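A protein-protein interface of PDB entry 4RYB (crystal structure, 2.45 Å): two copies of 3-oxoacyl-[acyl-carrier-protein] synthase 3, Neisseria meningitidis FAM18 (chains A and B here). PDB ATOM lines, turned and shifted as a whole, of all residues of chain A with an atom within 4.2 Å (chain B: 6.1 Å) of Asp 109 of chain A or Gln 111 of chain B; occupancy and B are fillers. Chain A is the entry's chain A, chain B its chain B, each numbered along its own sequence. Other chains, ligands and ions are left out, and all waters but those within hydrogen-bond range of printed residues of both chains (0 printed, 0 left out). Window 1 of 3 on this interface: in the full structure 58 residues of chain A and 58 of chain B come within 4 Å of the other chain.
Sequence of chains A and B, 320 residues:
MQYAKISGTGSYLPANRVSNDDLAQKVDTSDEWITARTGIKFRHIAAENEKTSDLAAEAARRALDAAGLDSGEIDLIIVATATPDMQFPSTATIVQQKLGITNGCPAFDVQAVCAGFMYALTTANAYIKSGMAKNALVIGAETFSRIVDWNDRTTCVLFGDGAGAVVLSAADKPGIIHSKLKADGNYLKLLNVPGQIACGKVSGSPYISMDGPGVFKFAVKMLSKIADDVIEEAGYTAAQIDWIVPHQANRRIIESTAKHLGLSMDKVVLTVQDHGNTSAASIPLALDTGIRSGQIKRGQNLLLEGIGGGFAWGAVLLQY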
ATOM      1  N   VAL A  79      15.738 -29.364  14.936  1.00  0.00           N
ATOM      2  CA  VAL A  79      16.861 -29.442  14.012  1.00  0.00           C
ATOM      3  C   VAL A  79      17.935 -30.365  14.580  1.00  0.00           C
ATOM      4  O   VAL A  79      18.417 -30.156  15.689  1.00  0.00           O
ATOM      5  CB  VAL A  79      17.460 -28.050  13.737  1.00  0.00           C
ATOM      6  CG1 VAL A  79      18.721 -28.157  12.884  1.00  0.00           C
ATOM      7  CG2 VAL A  79      16.434 -27.155  13.064  1.00  0.00           C
ATOM      8  N   THR A  81      21.672 -31.303  14.162  1.00  0.00           N
ATOM      9  CA  THR A  81      22.898 -30.799  13.553  1.00  0.00           C
ATOM     10  C   THR A  81      24.082 -30.937  14.503  1.00  0.00           C
ATOM     11  O   THR A  81      23.927 -30.869  15.724  1.00  0.00           O
ATOM     12  CB  THR A  81      22.753 -29.316  13.128  1.00  0.00           C
ATOM     13  OG1 THR A  81      23.956 -28.876  12.485  1.00  0.00           O
ATOM     14  CG2 THR A  81      22.467 -28.420  14.331  1.00  0.00           C
ATOM     15  N   GLN A  87      27.274 -20.885  19.064  1.00  0.00           N
ATOM     16  CA  GLN A  87      27.375 -21.584  20.336  1.00  0.00           C
ATOM     17  C   GLN A  87      25.977 -21.648  20.938  1.00  0.00           C
ATOM     18  O   GLN A  87      25.509 -22.712  21.348  1.00  0.00           O
ATOM     19  CB  GLN A  87      28.354 -20.875  21.269  1.00  0.00           C
ATOM     20  CG  GLN A  87      28.569 -21.575  22.598  1.00  0.00           C
ATOM     21  CD  GLN A  87      29.315 -22.883  22.449  1.00  0.00           C
ATOM     22  OE1 GLN A  87      30.209 -23.013  21.613  1.00  0.00           O
ATOM     23  NE2 GLN A  87      28.945 -23.866  23.259  1.00  0.00           N
ATOM     24  N   PHE A  88      25.315 -20.494  20.964  1.00  0.00           N
ATOM     25  CA  PHE A  88      23.881 -20.420  21.218  1.00  0.00           C
ATOM     26  C   PHE A  88      23.409 -19.034  20.760  1.00  0.00           C
ATOM     27  O   PHE A  88      24.231 -18.135  20.578  1.00  0.00           O
ATOM     28  CB  PHE A  88      23.548 -20.705  22.700  1.00  0.00           C
ATOM     29  CG  PHE A  88      23.778 -19.546  23.644  1.00  0.00           C
ATOM     30  CD1 PHE A  88      22.924 -18.448  23.657  1.00  0.00           C
ATOM     31  CD2 PHE A  88      24.800 -19.595  24.578  1.00  0.00           C
ATOM     32  CE1 PHE A  88      23.123 -17.403  24.545  1.00  0.00           C
ATOM     33  CE2 PHE A  88      24.997 -18.555  25.472  1.00  0.00           C
ATOM     34  CZ  PHE A  88      24.156 -17.458  25.454  1.00  0.00           C
ATOM     35  N   SER A  90      19.816 -21.662  19.787  1.00  0.00           N
ATOM     36  CA  SER A  90      19.583 -22.818  18.932  1.00  0.00           C
ATOM     37  C   SER A  90      19.493 -22.481  17.442  1.00  0.00           C
ATOM     38  O   SER A  90      19.003 -21.416  17.061  1.00  0.00           O
ATOM     39  CB  SER A  90      18.290 -23.503  19.373  1.00  0.00           C
ATOM     40  OG  SER A  90      18.073 -24.703  18.662  1.00  0.00           O
ATOM     41  N   THR A  91      19.995 -23.388  16.606  1.00  0.00           N
ATOM     42  CA  THR A  91      19.857 -23.259  15.159  1.00  0.00           C
ATOM     43  C   THR A  91      18.387 -23.354  14.764  1.00  0.00           C
ATOM     44  O   THR A  91      17.957 -22.749  13.783  1.00  0.00           O
ATOM     45  CB  THR A  91      20.668 -24.342  14.406  1.00  0.00           C
ATOM     46  OG1 THR A  91      22.067 -24.140  14.630  1.00  0.00           O
ATOM     47  CG2 THR A  91      20.399 -24.291  12.905  1.00  0.00           C
ATOM     48  N   ALA A  92      17.621 -24.117  15.538  1.00  0.00           N
ATOM     49  CA  ALA A  92      16.200 -24.299  15.270  1.00  0.00           C
ATOM     50  C   ALA A  92      15.453 -22.970  15.349  1.00  0.00           C
ATOM     51  O   ALA A  92      14.572 -22.697  14.531  1.00  0.00           O
ATOM     52  CB  ALA A  92      15.604 -25.305  16.244  1.00  0.00           C
ATOM     53  N   PHE A 108      14.070 -26.269  19.041  1.00  0.00           N
ATOM     54  CA  PHE A 108      15.336 -26.623  19.675  1.00  0.00           C
ATOM     55  C   PHE A 108      16.150 -27.600  18.833  1.00  0.00           C
ATOM     56  O   PHE A 108      15.612 -28.275  17.959  1.00  0.00           O
ATOM     57  CB  PHE A 108      15.078 -27.227  21.056  1.00  0.00           C
ATOM     58  CG  PHE A 108      14.302 -28.516  21.024  1.00  0.00           C
ATOM     59  CD1 PHE A 108      12.919 -28.511  20.942  1.00  0.00           C
ATOM     60  CD2 PHE A 108      14.958 -29.734  21.099  1.00  0.00           C
ATOM     61  CE1 PHE A 108      12.207 -29.696  20.922  1.00  0.00           C
ATOM     62  CE2 PHE A 108      14.249 -30.923  21.082  1.00  0.00           C
ATOM     63  CZ  PHE A 108      12.874 -30.905  20.993  1.00  0.00           C
ATOM     64  N   ASP A 109      17.449 -27.672  19.112  1.00  0.00           N
ATOM     65  CA  ASP A 109      18.331 -28.590  18.402  1.00  0.00           C
ATOM     66  C   ASP A 109      18.492 -29.893  19.166  1.00  0.00           C
ATOM     67  O   ASP A 109      18.418 -29.914  20.396  1.00  0.00           O
ATOM     68  CB  ASP A 109      19.712 -27.968  18.170  1.00  0.00           C
ATOM     69  CG  ASP A 109      19.668 -26.752  17.268  1.00  0.00           C
ATOM     70  OD1 ASP A 109      18.616 -26.511  16.634  1.00  0.00           O
ATOM     71  OD2 ASP A 109      20.689 -26.033  17.191  1.00  0.00           O
ATOM     72  N   VAL A 110      18.710 -30.975  18.422  1.00  0.00           N
ATOM     73  CA  VAL A 110      19.084 -32.258  19.002  1.00  0.00           C
ATOM     74  C   VAL A 110      20.468 -32.639  18.491  1.00  0.00           C
ATOM     75  O   VAL A 110      20.758 -32.494  17.303  1.00  0.00           O
ATOM     76  CB  VAL A 110      18.062 -33.366  18.649  1.00  0.00           C
ATOM     77  CG1 VAL A 110      18.625 -34.754  18.953  1.00  0.00           C
ATOM     78  CG2 VAL A 110      16.758 -33.145  19.394  1.00  0.00           C
ATOM     79  N   VAL B  79      20.594 -34.441  28.044  1.00  0.00           N
ATOM     80  CA  VAL B  79      21.348 -33.343  28.641  1.00  0.00           C
ATOM     81  C   VAL B  79      21.016 -32.020  27.956  1.00  0.00           C
ATOM     82  O   VAL B  79      21.149 -31.890  26.743  1.00  0.00           O
ATOM     83  CB  VAL B  79      22.870 -33.599  28.558  1.00  0.00           C
ATOM     84  CG1 VAL B  79      23.659 -32.392  29.069  1.00  0.00           C
ATOM     85  CG2 VAL B  79      23.244 -34.848  29.341  1.00  0.00           C
ATOM     86  N   ALA B  80      20.579 -31.042  28.741  1.00  0.00           N
ATOM     87  CA  ALA B  80      20.378 -29.690  28.236  1.00  0.00           C
ATOM     88  C   ALA B  80      21.602 -28.835  28.550  1.00  0.00           C
ATOM     89  O   ALA B  80      21.945 -28.635  29.715  1.00  0.00           O
ATOM     90  CB  ALA B  80      19.125 -29.073  28.838  1.00  0.00           C
ATOM     91  N   THR B  81      22.264 -28.344  27.507  1.00  0.00           N
ATOM     92  CA  THR B  81      23.458 -27.527  27.686  1.00  0.00           C
ATOM     93  C   THR B  81      23.711 -26.601  26.501  1.00  0.00           C
ATOM     94  O   THR B  81      23.369 -26.920  25.362  1.00  0.00           O
ATOM     95  CB  THR B  81      24.705 -28.406  27.907  1.00  0.00           C
ATOM     96  OG1 THR B  81      25.851 -27.575  28.135  1.00  0.00           O
ATOM     97  CG2 THR B  81      24.960 -29.306  26.702  1.00  0.00           C
ATOM     98  N   ALA B  82      24.293 -25.441  26.791  1.00  0.00           N
ATOM     99  CA  ALA B  82      24.725 -24.498  25.768  1.00  0.00           C
ATOM    100  C   ALA B  82      26.249 -24.433  25.734  1.00  0.00           C
ATOM    101  O   ALA B  82      26.831 -23.581  25.065  1.00  0.00           O
ATOM    102  CB  ALA B  82      24.137 -23.119  26.029  1.00  0.00           C
ATOM    103  N   THR B  83      26.888 -25.338  26.471  1.00  0.00           N
ATOM    104  CA  THR B  83      28.342 -25.395  26.544  1.00  0.00           C
ATOM    105  C   THR B  83      28.823 -26.846  26.571  1.00  0.00           C
ATOM    106  O   THR B  83      29.387 -27.302  27.564  1.00  0.00           O
ATOM    107  CB  THR B  83      28.870 -24.657  27.791  1.00  0.00           C
ATOM    108  OG1 THR B  83      28.137 -25.078  28.947  1.00  0.00           O
ATOM    109  CG2 THR B  83      28.726 -23.151  27.624  1.00  0.00           C
ATOM    110  N   ASP B 109      21.851 -34.535  23.396  1.00  0.00           N
ATOM    111  CA  ASP B 109      21.772 -33.193  23.961  1.00  0.00           C
ATOM    112  C   ASP B 109      20.610 -32.409  23.367  1.00  0.00           C
ATOM    113  O   ASP B 109      20.233 -32.620  22.214  1.00  0.00           O
ATOM    114  CB  ASP B 109      23.067 -32.413  23.725  1.00  0.00           C
ATOM    115  CG  ASP B 109      24.265 -33.035  24.407  1.00  0.00           C
ATOM    116  OD1 ASP B 109      24.077 -33.932  25.255  1.00  0.00           O
ATOM    117  OD2 ASP B 109      25.401 -32.616  24.092  1.00  0.00           O
ATOM    118  N   VAL B 110      20.053 -31.506  24.169  1.00  0.00           N
ATOM    119  CA  VAL B 110      19.080 -30.529  23.693  1.00  0.00           C
ATOM    120  C   VAL B 110      19.620 -29.117  23.895  1.00  0.00           C
ATOM    121  O   VAL B 110      20.229 -28.817  24.922  1.00  0.00           O
ATOM    122  CB  VAL B 110      17.722 -30.683  24.409  1.00  0.00           C
ATOM    123  CG1 VAL B 110      16.834 -29.461  24.175  1.00  0.00           C
ATOM    124  CG2 VAL B 110      17.021 -31.947  23.944  1.00  0.00           C
ATOM    125  N   GLN B 111      19.394 -28.267  22.910  1.00  0.00           N
ATOM    126  CA  GLN B 111      19.830 -26.899  23.006  1.00  0.00           C
ATOM    127  C   GLN B 111      18.660 -25.925  23.025  1.00  0.00           C
ATOM    128  O   GLN B 111      18.040 -25.675  22.015  1.00  0.00           O
ATOM    129  CB  GLN B 111      20.756 -26.585  21.839  1.00  0.00           C
ATOM    130  CG  GLN B 111      20.970 -25.117  21.561  1.00  0.00           C
ATOM    131  CD  GLN B 111      21.739 -24.430  22.647  1.00  0.00           C
ATOM    132  OE1 GLN B 111      21.360 -24.460  23.802  1.00  0.00           O
ATOM    133  NE2 GLN B 111      22.829 -23.804  22.276  1.00  0.00           N
ATOM    134  N   ALA B 112      18.376 -25.393  24.206  1.00  0.00           N
ATOM    135  CA  ALA B 112      17.350 -24.386  24.398  1.00  0.00           C
ATOM    136  C   ALA B 112      17.853 -23.317  25.348  1.00  0.00           C
ATOM    137  O   ALA B 112      17.074 -22.532  25.865  1.00  0.00           O
ATOM    138  CB  ALA B 112      16.067 -24.995  24.913  1.00  0.00           C
ATOM    139  N   VAL B 113      19.158 -23.311  25.582  1.00  0.00           N
ATOM    140  CA  VAL B 113      19.814 -22.383  26.480  1.00  0.00           C
ATOM    141  C   VAL B 113      19.235 -22.431  27.889  1.00  0.00           C
ATOM    142  O   VAL B 113      19.119 -23.484  28.482  1.00  0.00           O
ATOM    143  CB  VAL B 113      19.839 -20.956  25.927  1.00  0.00           C
ATOM    144  CG1 VAL B 113      21.019 -20.208  26.497  1.00  0.00           C
ATOM    145  CG2 VAL B 113      19.951 -20.977  24.418  1.00  0.00           C
ATOM    146  N   GLY B 116      16.574 -24.796  28.655  1.00  0.00           N
ATOM    147  CA  GLY B 116      16.967 -26.147  28.296  1.00  0.00           C
ATOM    148  C   GLY B 116      16.358 -27.265  29.122  1.00  0.00           C
ATOM    149  O   GLY B 116      15.952 -28.291  28.571  1.00  0.00           O
ATOM    150  N   TYR B 119      12.690 -27.854  28.361  1.00  0.00           N
ATOM    151  CA  TYR B 119      12.590 -28.480  27.048  1.00  0.00           C
ATOM    152  C   TYR B 119      12.930 -29.962  27.144  1.00  0.00           C
ATOM    153  O   TYR B 119      12.265 -30.800  26.536  1.00  0.00           O
ATOM    154  CB  TYR B 119      13.519 -27.792  26.044  1.00  0.00           C
ATOM    155  CG  TYR B 119      12.843 -26.729  25.213  1.00  0.00           C
ATOM    156  CD1 TYR B 119      12.552 -25.481  25.749  1.00  0.00           C
ATOM    157  CD2 TYR B 119      12.494 -26.972  23.891  1.00  0.00           C
ATOM    158  CE1 TYR B 119      11.933 -24.505  24.991  1.00  0.00           C
ATOM    159  CE2 TYR B 119      11.875 -26.004  23.125  1.00  0.00           C
ATOM    160  CZ  TYR B 119      11.596 -24.771  23.680  1.00  0.00           C
ATOM    161  OH  TYR B 119      10.977 -23.803  22.921  1.00  0.00           O
ATOM    162  N   GLU B 142      25.902 -26.715  32.808  1.00  0.00           N
ATOM    163  CA  GLU B 142      26.507 -25.594  32.100  1.00  0.00           C
ATOM    164  C   GLU B 142      27.865 -25.193  32.679  1.00  0.00           C
ATOM    165  O   GLU B 142      28.100 -25.299  33.884  1.00  0.00           O
ATOM    166  CB  GLU B 142      25.557 -24.397  32.135  1.00  0.00           C
ATOM    167  CG  GLU B 142      24.185 -24.674  31.530  1.00  0.00           C
ATOM    168  CD  GLU B 142      24.161 -24.543  30.019  1.00  0.00           C
ATOM    169  OE1 GLU B 142      25.243 -24.552  29.397  1.00  0.00           O
ATOM    170  OE2 GLU B 142      23.051 -24.424  29.455  1.00  0.00           O
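The backbone carbonyl oxygen (O) of Ala 82 of chain B sits at hydrogen-bond distance from the side-chain amide nitrogen (NE2) of Gln 87 of chain A (2.8 Å). The backbone carbonyl oxygen (O) of Gln 87 of chain A lies within hydrogen-bond range of the side-chain amide nitrogen (NE2) of Gln 111 of chain B, 3.0 Å away. The backbone carbonyl oxygen (O) of Gln 111 of chain B sits close to the side-chain hydroxyl (OG) of Ser 90 of chain A, at 3.5 Å. The backbone carbonyl oxygen (O) of Asp 109 of chain A is in hydrogen-bond range of the backbone NH (N) of Gln 111 of chain B, 3.2 Å away.
N of Val 110 of chain A lies within hydrogen-bond range of O of Val 79 of chain A. The backbone NH (N) of Thr 91 of chain A is in hydrogen-bond range of the side-chain carboxylate (OD2) of Asp 109 of chain A (2.8 Å). The backbone NH of Val 110 of chain B sits at hydrogen-bond distance from the backbone carbonyl oxygen of Val 79 of chain B (2.8 Å). The backbone NH of Thr 83 of chain B sits at hydrogen-bond distance from the side-chain hydroxyl of Thr 81 of chain B (3.0 Å). The backbone carbonyl oxygen (O) of Val 110 of chain B is in hydrogen-bond range of the backbone NH (N) of Thr 81 of chain B (3.3 Å). N of Ala 82 of chain B sits at hydrogen-bond distance from OE1 of Glu 142 of chain B, at 2.9 Å.
NE2 of Gln 87 of chain A touches CA of Thr 83 of chain B, at 3.7 Å. Phe 88 of chain A touches Ala 82 of chain B (CD2 to CB, 3.9 Å). Gln 111 of chain B touches Phe 88 of chain A. CD1 of Phe 88 of chain A touches CG1 of Val 113 of chain B, 3.8 Å away. Val 110 of chain B touches Phe 108 of chain A. Phe 108 of chain A touches Gln 111 of chain B (CB to O, 3.5 Å). Phe 108 of chain A touches Tyr 119 of chain B (CD1 to CD2, 3.4 Å). Asp 109 of chain A touches Asp 109 of chain B (O to O, 3.7 Å). Asp 109 of chain A touches Val 110 of chain B. CA of Val 110 of chain A touches O of Asp 109 of chain B (3.4 Å).
Val 79 of chain A touches none of the printed residues of chain B. Ala 92 of chain A touches none of the printed residues of chain B. Asp 109 of chain A touches three residues of chain B. Of the printed residues of chain A, Thr 83 of chain B touches Gln 87. Gln 111 of chain B touches five residues of chain A. Printed residues of chain A within 4 Å of Val 113 of chain B: Phe 88. Of the printed residues of chain A, Tyr 119 of chain B touches Phe 108. The nearest residue of chain B that does not touch Asp 109 of chain A is Ala 112 of chain B (5.7 Å). The nearest printed residue of chain A that does not touch Val 110 of chain B is Val 110 of chain A (4.7 Å).
Hydrophobic or aromatic side chains of chain B that line the printed part of chain A: Ala 82, Val 110, Val 113 and Tyr 119. Of the 10 printed residues of chain A, 6 touch a printed residue of chain B. Hydrophobic or aromatic side chains of chain A within 4 Å of the printed part of chain B: Phe 88 and Phe 108.
Asp 109 of chain B touches its own counterpart, Asp 109 of chain A. Asp 109 of chain A touches Val 110 of chain B, and with the chains exchanged Val 110 of chain A touches Asp 109 of chain B.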
